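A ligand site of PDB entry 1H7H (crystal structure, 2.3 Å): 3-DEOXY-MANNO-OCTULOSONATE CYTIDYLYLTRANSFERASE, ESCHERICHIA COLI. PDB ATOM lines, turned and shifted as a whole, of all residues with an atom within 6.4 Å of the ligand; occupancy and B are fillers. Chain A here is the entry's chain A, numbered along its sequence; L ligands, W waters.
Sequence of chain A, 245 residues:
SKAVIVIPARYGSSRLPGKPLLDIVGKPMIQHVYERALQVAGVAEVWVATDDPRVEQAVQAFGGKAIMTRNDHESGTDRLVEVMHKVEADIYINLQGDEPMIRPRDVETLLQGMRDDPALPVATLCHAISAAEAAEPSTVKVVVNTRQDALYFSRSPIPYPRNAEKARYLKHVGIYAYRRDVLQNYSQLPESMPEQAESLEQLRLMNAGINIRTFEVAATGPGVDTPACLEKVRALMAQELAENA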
ATOM      1  N   ILE A   7      29.579 -25.234  15.015  1.00  0.00           N
ATOM      2  CA  ILE A   7      30.298 -24.269  15.834  1.00  0.00           C
ATOM      3  C   ILE A   7      29.311 -23.263  16.416  1.00  0.00           C
ATOM      4  O   ILE A   7      28.870 -22.358  15.717  1.00  0.00           O
ATOM      5  CB  ILE A   7      31.322 -23.485  14.993  1.00  0.00           C
ATOM      6  CG1 ILE A   7      32.340 -24.449  14.365  1.00  0.00           C
ATOM      7  CG2 ILE A   7      32.041 -22.431  15.842  1.00  0.00           C
ATOM      8  CD1 ILE A   7      33.097 -23.846  13.229  1.00  0.00           C
ATOM      9  N   PRO A   8      28.901 -23.447  17.680  1.00  0.00           N
ATOM     10  CA  PRO A   8      27.965 -22.525  18.319  1.00  0.00           C
ATOM     11  C   PRO A   8      28.677 -21.189  18.531  1.00  0.00           C
ATOM     12  O   PRO A   8      29.774 -21.154  19.099  1.00  0.00           O
ATOM     13  CB  PRO A   8      27.658 -23.193  19.670  1.00  0.00           C
ATOM     14  CG  PRO A   8      27.956 -24.645  19.437  1.00  0.00           C
ATOM     15  CD  PRO A   8      29.180 -24.615  18.553  1.00  0.00           C
ATOM     16  N   ALA A   9      28.086 -20.104  18.049  1.00  0.00           N
ATOM     17  CA  ALA A   9      28.712 -18.797  18.179  1.00  0.00           C
ATOM     18  C   ALA A   9      27.729 -17.701  18.575  1.00  0.00           C
ATOM     19  O   ALA A   9      27.132 -17.026  17.744  1.00  0.00           O
ATOM     20  CB  ALA A   9      29.428 -18.415  16.886  1.00  0.00           C
ATOM     21  N   ARG A  10      27.598 -17.556  19.894  1.00  0.00           N
ATOM     22  CA  ARG A  10      26.726 -16.565  20.506  1.00  0.00           C
ATOM     23  C   ARG A  10      27.496 -15.246  20.551  1.00  0.00           C
ATOM     24  O   ARG A  10      28.686 -15.212  20.890  1.00  0.00           O
ATOM     25  CB  ARG A  10      26.402 -17.030  21.928  1.00  0.00           C
ATOM     26  CG  ARG A  10      25.149 -16.450  22.519  1.00  0.00           C
ATOM     27  CD  ARG A  10      25.006 -16.866  23.965  1.00  0.00           C
ATOM     28  NE  ARG A  10      23.675 -16.586  24.503  1.00  0.00           N
ATOM     29  CZ  ARG A  10      23.368 -16.555  25.801  1.00  0.00           C
ATOM     30  NH1 ARG A  10      24.304 -16.777  26.700  1.00  0.00           N
ATOM     31  NH2 ARG A  10      22.125 -16.327  26.177  1.00  0.00           N
ATOM     32  N   TYR A  11      26.829 -14.154  20.165  1.00  0.00           N
ATOM     33  CA  TYR A  11      27.441 -12.828  20.157  1.00  0.00           C
ATOM     34  C   TYR A  11      27.565 -12.298  21.581  1.00  0.00           C
ATOM     35  O   TYR A  11      28.679 -11.974  22.041  1.00  0.00           O
ATOM     36  CB  TYR A  11      26.588 -11.856  19.325  1.00  0.00           C
ATOM     37  CG  TYR A  11      27.164 -10.454  19.184  1.00  0.00           C
ATOM     38  CD1 TYR A  11      27.849 -10.063  18.033  1.00  0.00           C
ATOM     39  CD2 TYR A  11      27.006  -9.516  20.203  1.00  0.00           C
ATOM     40  CE1 TYR A  11      28.363  -8.767  17.893  1.00  0.00           C
ATOM     41  CE2 TYR A  11      27.516  -8.224  20.076  1.00  0.00           C
ATOM     42  CZ  TYR A  11      28.185  -7.857  18.919  1.00  0.00           C
ATOM     43  OH  TYR A  11      28.705  -6.585  18.796  1.00  0.00           O
ATOM     44  N   GLY A  12      26.429 -12.222  22.272  1.00  0.00           N
ATOM     45  CA  GLY A  12      26.376 -11.732  23.638  1.00  0.00           C
ATOM     46  C   GLY A  12      27.362 -12.355  24.611  1.00  0.00           C
ATOM     47  O   GLY A  12      27.276 -13.541  24.925  1.00  0.00           O
ATOM     48  N   SER A  13      28.278 -11.537  25.091  1.00  0.00           N
ATOM     49  CA  SER A  13      29.296 -11.965  26.054  1.00  0.00           C
ATOM     50  C   SER A  13      29.615 -10.781  26.973  1.00  0.00           C
ATOM     51  O   SER A  13      29.773  -9.645  26.516  1.00  0.00           O
ATOM     52  CB  SER A  13      30.553 -12.442  25.312  1.00  0.00           C
ATOM     53  OG  SER A  13      31.501 -13.004  26.209  1.00  0.00           O
ATOM     54  N   SER A  14      29.661 -11.059  28.266  1.00  0.00           N
ATOM     55  CA  SER A  14      29.922 -10.037  29.292  1.00  0.00           C
ATOM     56  C   SER A  14      31.244  -9.284  29.175  1.00  0.00           C
ATOM     57  O   SER A  14      31.259  -8.093  28.841  1.00  0.00           O
ATOM     58  CB  SER A  14      29.798 -10.671  30.687  1.00  0.00           C
ATOM     59  OG  SER A  14      30.572 -11.865  30.784  1.00  0.00           O
ATOM     60  N   LYS A  19      32.296 -11.496  20.904  1.00  0.00           N
ATOM     61  CA  LYS A  19      33.530 -12.255  20.983  1.00  0.00           C
ATOM     62  C   LYS A  19      33.950 -12.936  19.672  1.00  0.00           C
ATOM     63  O   LYS A  19      35.108 -12.841  19.278  1.00  0.00           O
ATOM     64  CB  LYS A  19      33.449 -13.267  22.132  1.00  0.00           C
ATOM     65  CG  LYS A  19      34.759 -13.943  22.495  1.00  0.00           C
ATOM     66  CD  LYS A  19      34.670 -14.670  23.831  1.00  0.00           C
ATOM     67  CE  LYS A  19      33.594 -15.749  23.828  1.00  0.00           C
ATOM     68  NZ  LYS A  19      33.561 -16.473  25.135  1.00  0.00           N
ATOM     69  N   ALA A  49      26.237 -22.215  14.295  1.00  0.00           N
ATOM     70  CA  ALA A  49      24.927 -22.030  14.893  1.00  0.00           C
ATOM     71  C   ALA A  49      24.960 -20.731  15.686  1.00  0.00           C
ATOM     72  O   ALA A  49      25.807 -20.567  16.563  1.00  0.00           O
ATOM     73  CB  ALA A  49      24.598 -23.199  15.806  1.00  0.00           C
ATOM     74  N   ASP A  51      22.562 -17.038  17.269  1.00  0.00           N
ATOM     75  CA  ASP A  51      21.293 -16.411  17.646  1.00  0.00           C
ATOM     76  C   ASP A  51      21.278 -14.923  17.287  1.00  0.00           C
ATOM     77  O   ASP A  51      20.253 -14.253  17.442  1.00  0.00           O
ATOM     78  CB  ASP A  51      21.015 -16.613  19.147  1.00  0.00           C
ATOM     79  CG  ASP A  51      22.099 -16.011  20.063  1.00  0.00           C
ATOM     80  OD1 ASP A  51      23.205 -15.664  19.582  1.00  0.00           O
ATOM     81  OD2 ASP A  51      21.835 -15.893  21.279  1.00  0.00           O
ATOM     82  N   ASN A  71      17.327 -17.795  20.756  1.00  0.00           N
ATOM     83  CA  ASN A  71      18.179 -17.094  21.721  1.00  0.00           C
ATOM     84  C   ASN A  71      17.888 -17.532  23.162  1.00  0.00           C
ATOM     85  O   ASN A  71      18.665 -17.248  24.073  1.00  0.00           O
ATOM     86  CB  ASN A  71      18.039 -15.576  21.574  1.00  0.00           C
ATOM     87  CG  ASN A  71      16.585 -15.120  21.536  1.00  0.00           C
ATOM     88  OD1 ASN A  71      16.115 -14.597  20.515  1.00  0.00           O
ATOM     89  ND2 ASN A  71      15.861 -15.307  22.636  1.00  0.00           N
ATOM     90  N   HIS A  73      18.084 -20.394  24.280  1.00  0.00           N
ATOM     91  CA  HIS A  73      18.895 -21.578  24.563  1.00  0.00           C
ATOM     92  C   HIS A  73      19.796 -21.294  25.760  1.00  0.00           C
ATOM     93  O   HIS A  73      20.521 -20.293  25.778  1.00  0.00           O
ATOM     94  CB  HIS A  73      19.766 -21.952  23.351  1.00  0.00           C
ATOM     95  CG  HIS A  73      19.063 -22.789  22.332  1.00  0.00           C
ATOM     96  ND1 HIS A  73      18.171 -23.776  22.670  1.00  0.00           N
ATOM     97  CD2 HIS A  73      19.147 -22.800  20.980  1.00  0.00           C
ATOM     98  CE1 HIS A  73      17.737 -24.360  21.569  1.00  0.00           C
ATOM     99  NE2 HIS A  73      18.316 -23.782  20.533  1.00  0.00           N
ATOM    100  N   GLU A  74      19.763 -22.195  26.735  1.00  0.00           N
ATOM    101  CA  GLU A  74      20.575 -22.034  27.934  1.00  0.00           C
ATOM    102  C   GLU A  74      22.030 -22.487  27.779  1.00  0.00           C
ATOM    103  O   GLU A  74      22.910 -22.059  28.537  1.00  0.00           O
ATOM    104  CB  GLU A  74      19.904 -22.704  29.144  1.00  0.00           C
ATOM    105  CG  GLU A  74      19.321 -24.072  28.874  1.00  0.00           C
ATOM    106  CD  GLU A  74      18.474 -24.610  30.029  1.00  0.00           C
ATOM    107  OE1 GLU A  74      18.979 -24.641  31.187  1.00  0.00           O
ATOM    108  OE2 GLU A  74      17.318 -25.011  29.787  1.00  0.00           O
ATOM    109  N   SER A  75      22.316 -23.288  26.752  1.00  0.00           N
ATOM    110  CA  SER A  75      23.670 -23.798  26.532  1.00  0.00           C
ATOM    111  C   SER A  75      23.986 -24.157  25.088  1.00  0.00           C
ATOM    112  O   SER A  75      23.103 -24.186  24.231  1.00  0.00           O
ATOM    113  CB  SER A  75      23.922 -25.017  27.403  1.00  0.00           C
ATOM    114  OG  SER A  75      23.046 -26.063  27.029  1.00  0.00           O
ATOM    115  N   GLY A  76      25.252 -24.462  24.841  1.00  0.00           N
ATOM    116  CA  GLY A  76      25.684 -24.833  23.505  1.00  0.00           C
ATOM    117  C   GLY A  76      25.190 -26.200  23.077  1.00  0.00           C
ATOM    118  O   GLY A  76      25.230 -26.511  21.892  1.00  0.00           O
ATOM    119  N   THR A  77      24.773 -27.030  24.031  1.00  0.00           N
ATOM    120  CA  THR A  77      24.278 -28.359  23.708  1.00  0.00           C
ATOM    121  C   THR A  77      22.809 -28.311  23.305  1.00  0.00           C
ATOM    122  O   THR A  77      22.369 -29.062  22.440  1.00  0.00           O
ATOM    123  CB  THR A  77      24.501 -29.377  24.870  1.00  0.00           C
ATOM    124  OG1 THR A  77      25.902 -29.494  25.122  1.00  0.00           O
ATOM    125  CG2 THR A  77      23.972 -30.759  24.504  1.00  0.00           C
ATOM    126  N   ARG A  79      21.472 -25.804  21.817  1.00  0.00           N
ATOM    127  CA  ARG A  79      21.554 -25.180  20.499  1.00  0.00           C
ATOM    128  C   ARG A  79      21.885 -26.225  19.427  1.00  0.00           C
ATOM    129  O   ARG A  79      21.375 -26.155  18.320  1.00  0.00           O
ATOM    130  CB  ARG A  79      22.588 -24.056  20.528  1.00  0.00           C
ATOM    131  CG  ARG A  79      22.911 -23.426  19.176  1.00  0.00           C
ATOM    132  CD  ARG A  79      23.703 -22.117  19.334  1.00  0.00           C
ATOM    133  NE  ARG A  79      22.827 -20.962  19.533  1.00  0.00           N
ATOM    134  CZ  ARG A  79      22.463 -20.471  20.720  1.00  0.00           C
ATOM    135  NH1 ARG A  79      22.910 -21.025  21.841  1.00  0.00           N
ATOM    136  NH2 ARG A  79      21.606 -19.460  20.785  1.00  0.00           N
ATOM    137  N   ASN A  94      30.876 -30.843  18.307  1.00  0.00           N
ATOM    138  CA  ASN A  94      30.655 -29.515  18.839  1.00  0.00           C
ATOM    139  C   ASN A  94      31.976 -28.811  19.101  1.00  0.00           C
ATOM    140  O   ASN A  94      32.752 -29.242  19.951  1.00  0.00           O
ATOM    141  CB  ASN A  94      29.851 -29.602  20.134  1.00  0.00           C
ATOM    142  CG  ASN A  94      29.103 -28.326  20.436  1.00  0.00           C
ATOM    143  OD1 ASN A  94      28.465 -27.758  19.550  1.00  0.00           O
ATOM    144  ND2 ASN A  94      29.155 -27.892  21.676  1.00  0.00           N
ATOM    145  N   LEU A  95      32.250 -27.760  18.341  1.00  0.00           N
ATOM    146  CA  LEU A  95      33.480 -26.983  18.499  1.00  0.00           C
ATOM    147  C   LEU A  95      33.166 -25.637  19.103  1.00  0.00           C
ATOM    148  O   LEU A  95      32.151 -25.016  18.764  1.00  0.00           O
ATOM    149  CB  LEU A  95      34.147 -26.743  17.152  1.00  0.00           C
ATOM    150  CG  LEU A  95      34.993 -27.834  16.523  1.00  0.00           C
ATOM    151  CD1 LEU A  95      35.724 -27.213  15.322  1.00  0.00           C
ATOM    152  CD2 LEU A  95      35.996 -28.342  17.531  1.00  0.00           C
ATOM    153  N   GLN A  96      34.048 -25.148  19.967  1.00  0.00           N
ATOM    154  CA  GLN A  96      33.870 -23.856  20.609  1.00  0.00           C
ATOM    155  C   GLN A  96      34.185 -22.728  19.631  1.00  0.00           C
ATOM    156  O   GLN A  96      35.209 -22.754  18.946  1.00  0.00           O
ATOM    157  CB  GLN A  96      34.778 -23.757  21.831  1.00  0.00           C
ATOM    158  CG  GLN A  96      34.565 -24.889  22.823  1.00  0.00           C
ATOM    159  CD  GLN A  96      33.190 -24.850  23.453  1.00  0.00           C
ATOM    160  OE1 GLN A  96      33.018 -24.298  24.547  1.00  0.00           O
ATOM    161  NE2 GLN A  96      32.187 -25.408  22.770  1.00  0.00           N
ATOM    162  N   GLY A  97      33.317 -21.727  19.588  1.00  0.00           N
ATOM    163  CA  GLY A  97      33.537 -20.616  18.692  1.00  0.00           C
ATOM    164  C   GLY A  97      34.617 -19.656  19.145  1.00  0.00           C
ATOM    165  O   GLY A  97      35.063 -18.806  18.370  1.00  0.00           O
ATOM    166  N   ASP A  98      35.060 -19.802  20.393  1.00  0.00           N
ATOM    167  CA  ASP A  98      36.080 -18.923  20.972  1.00  0.00           C
ATOM    168  C   ASP A  98      37.474 -19.529  21.151  1.00  0.00           C
ATOM    169  O   ASP A  98      38.320 -18.960  21.860  1.00  0.00           O
ATOM    170  CB  ASP A  98      35.589 -18.320  22.290  1.00  0.00           C
ATOM    171  CG  ASP A  98      35.317 -19.374  23.375  1.00  0.00           C
ATOM    172  OD1 ASP A  98      35.521 -20.584  23.133  1.00  0.00           O
ATOM    173  OD2 ASP A  98      34.902 -18.964  24.480  1.00  0.00           O
ATOM    174  N   VAL A 224      40.117 -17.860  24.538  1.00  0.00           N
ATOM    175  CA  VAL A 224      39.897 -16.428  24.595  1.00  0.00           C
ATOM    176  C   VAL A 224      38.720 -16.035  25.480  1.00  0.00           C
ATOM    177  O   VAL A 224      37.554 -16.229  25.125  1.00  0.00           O
ATOM    178  CB  VAL A 224      39.689 -15.824  23.175  1.00  0.00           C
ATOM    179  CG1 VAL A 224      39.400 -14.334  23.260  1.00  0.00           C
ATOM    180  CG2 VAL A 224      40.939 -16.073  22.321  1.00  0.00           C
ATOM    181  N   ASP A 225      39.031 -15.474  26.653  1.00  0.00           N
ATOM    182  CA  ASP A 225      38.044 -15.021  27.616  1.00  0.00           C
ATOM    183  C   ASP A 225      38.512 -13.718  28.232  1.00  0.00           C
ATOM    184  O   ASP A 225      37.721 -12.834  28.545  1.00  0.00           O
ATOM    185  CB  ASP A 225      37.820 -16.064  28.712  1.00  0.00           C
ATOM    186  CG  ASP A 225      37.017 -17.265  28.231  1.00  0.00           C
ATOM    187  OD1 ASP A 225      35.821 -17.091  27.913  1.00  0.00           O
ATOM    188  OD2 ASP A 225      37.581 -18.375  28.162  1.00  0.00           O
HETATM  189  O1  LIG L   1      28.590 -18.018  26.717  1.00  0.00           O
HETATM  190  P1  LIG L   1      30.201 -18.114  26.705  1.00  0.00           P
HETATM  191  O2  LIG L   1      30.674 -18.281  25.287  1.00  0.00           O
HETATM  192  O3  LIG L   1      30.765 -16.840  27.247  1.00  0.00           O
HETATM  193  O4  LIG L   1      30.678 -19.344  27.639  1.00  0.00           O
HETATM  194  P2  LIG L   1      31.499 -20.525  26.902  1.00  0.00           P
HETATM  195  O5  LIG L   1      31.882 -21.573  27.901  1.00  0.00           O
HETATM  196  O6  LIG L   1      32.746 -19.989  26.264  1.00  0.00           O
HETATM  197  O7  LIG L   1      30.589 -21.166  25.747  1.00  0.00           O
HETATM  198  C1  LIG L   1      30.983 -22.338  25.016  1.00  0.00           C
HETATM  199  C2  LIG L   1      30.527 -22.275  23.519  1.00  0.00           C
HETATM  200  O8  LIG L   1      29.101 -22.514  23.373  1.00  0.00           O
HETATM  201  C3  LIG L   1      30.779 -20.907  22.843  1.00  0.00           C
HETATM  202  O9  LIG L   1      31.054 -21.118  21.444  1.00  0.00           O
HETATM  203  C4  LIG L   1      29.441 -20.183  23.084  1.00  0.00           C
HETATM  204  O10 LIG L   1      29.195 -19.078  22.201  1.00  0.00           O
HETATM  205  C5  LIG L   1      28.375 -21.309  22.937  1.00  0.00           C
HETATM  206  N1  LIG L   1      27.134 -21.001  23.689  1.00  0.00           N
HETATM  207  C6  LIG L   1      25.936 -20.950  23.035  1.00  0.00           C
HETATM  208  O11 LIG L   1      25.820 -21.143  21.826  1.00  0.00           O
HETATM  209  N2  LIG L   1      24.715 -20.638  23.755  1.00  0.00           N
HETATM  210  C7  LIG L   1      24.710 -20.409  25.017  1.00  0.00           C
HETATM  211  N3  LIG L   1      23.605 -20.133  25.676  1.00  0.00           N
HETATM  212  C8  LIG L   1      26.025 -20.480  25.724  1.00  0.00           C
HETATM  213  C9  LIG L   1      27.160 -20.773  25.037  1.00  0.00           C
HETATM  214  O   HOH W   1      34.945 -21.438  25.620  1.00  0.00           O
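Water W1 bridges the side-chain carboxylate of Asp 98 (2.7 Å) and an oxygen (O6) of the ligand (2.7 Å).
The guanidinium group (NH2) of Arg 79 lies within salt-bridge range of the side-chain carboxylate (OD2) of Asp 51 (3.6 Å).
The side-chain carboxylate (OD2) of Asp 98 lies within salt-bridge range of the side-chain amino group (NZ) of Lys 19, at 2.9 Å.
The backbone carbonyl oxygen (O) of Asp 98 is in hydrogen-bond range of the backbone NH (N) of Val 224 (3.4 Å).
OD2 of Asp 51 is in salt-bridge range of NE of Arg 10 (3.8 Å).
The side-chain amino group of Lys 19 is in salt-bridge range of the side-chain carboxylate of Asp 225, at 3.6 Å.
N2 of the ligand lies within hydrogen-bond range of NH1 of Arg 79, 2.7 Å away.
The backbone carbonyl oxygen (O) of Pro 8 is in hydrogen-bond range of an oxygen (O9) of the ligand.
OD2 of Asp 98 lies close to O6 of the ligand (3.0 Å).
The backbone NH (N) of Gly 97 sits at hydrogen-bond distance from an oxygen (O9) of the ligand (3.0 Å).
The backbone carbonyl oxygen (O) of His 73 lies within hydrogen-bond range of a nitrogen (N3) of the ligand, at 3.1 Å.
O10 of the ligand sits at hydrogen-bond distance from N of Arg 10 (3.2 Å).
O2 of the ligand is in salt-bridge range of NZ of Lys 19, at 3.4 Å.
Residues that only touch the ligand: Glu 74 (3.5 Å), Ser 75 (3.6 Å), Gly 76 (3.9 Å) and Gln 96 (2.9 Å).
Hydrophobic or aromatic side chains that line the ligand: Pro 8.
Of the 25 residues printed, 11 come within 4 Å of the ligand.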
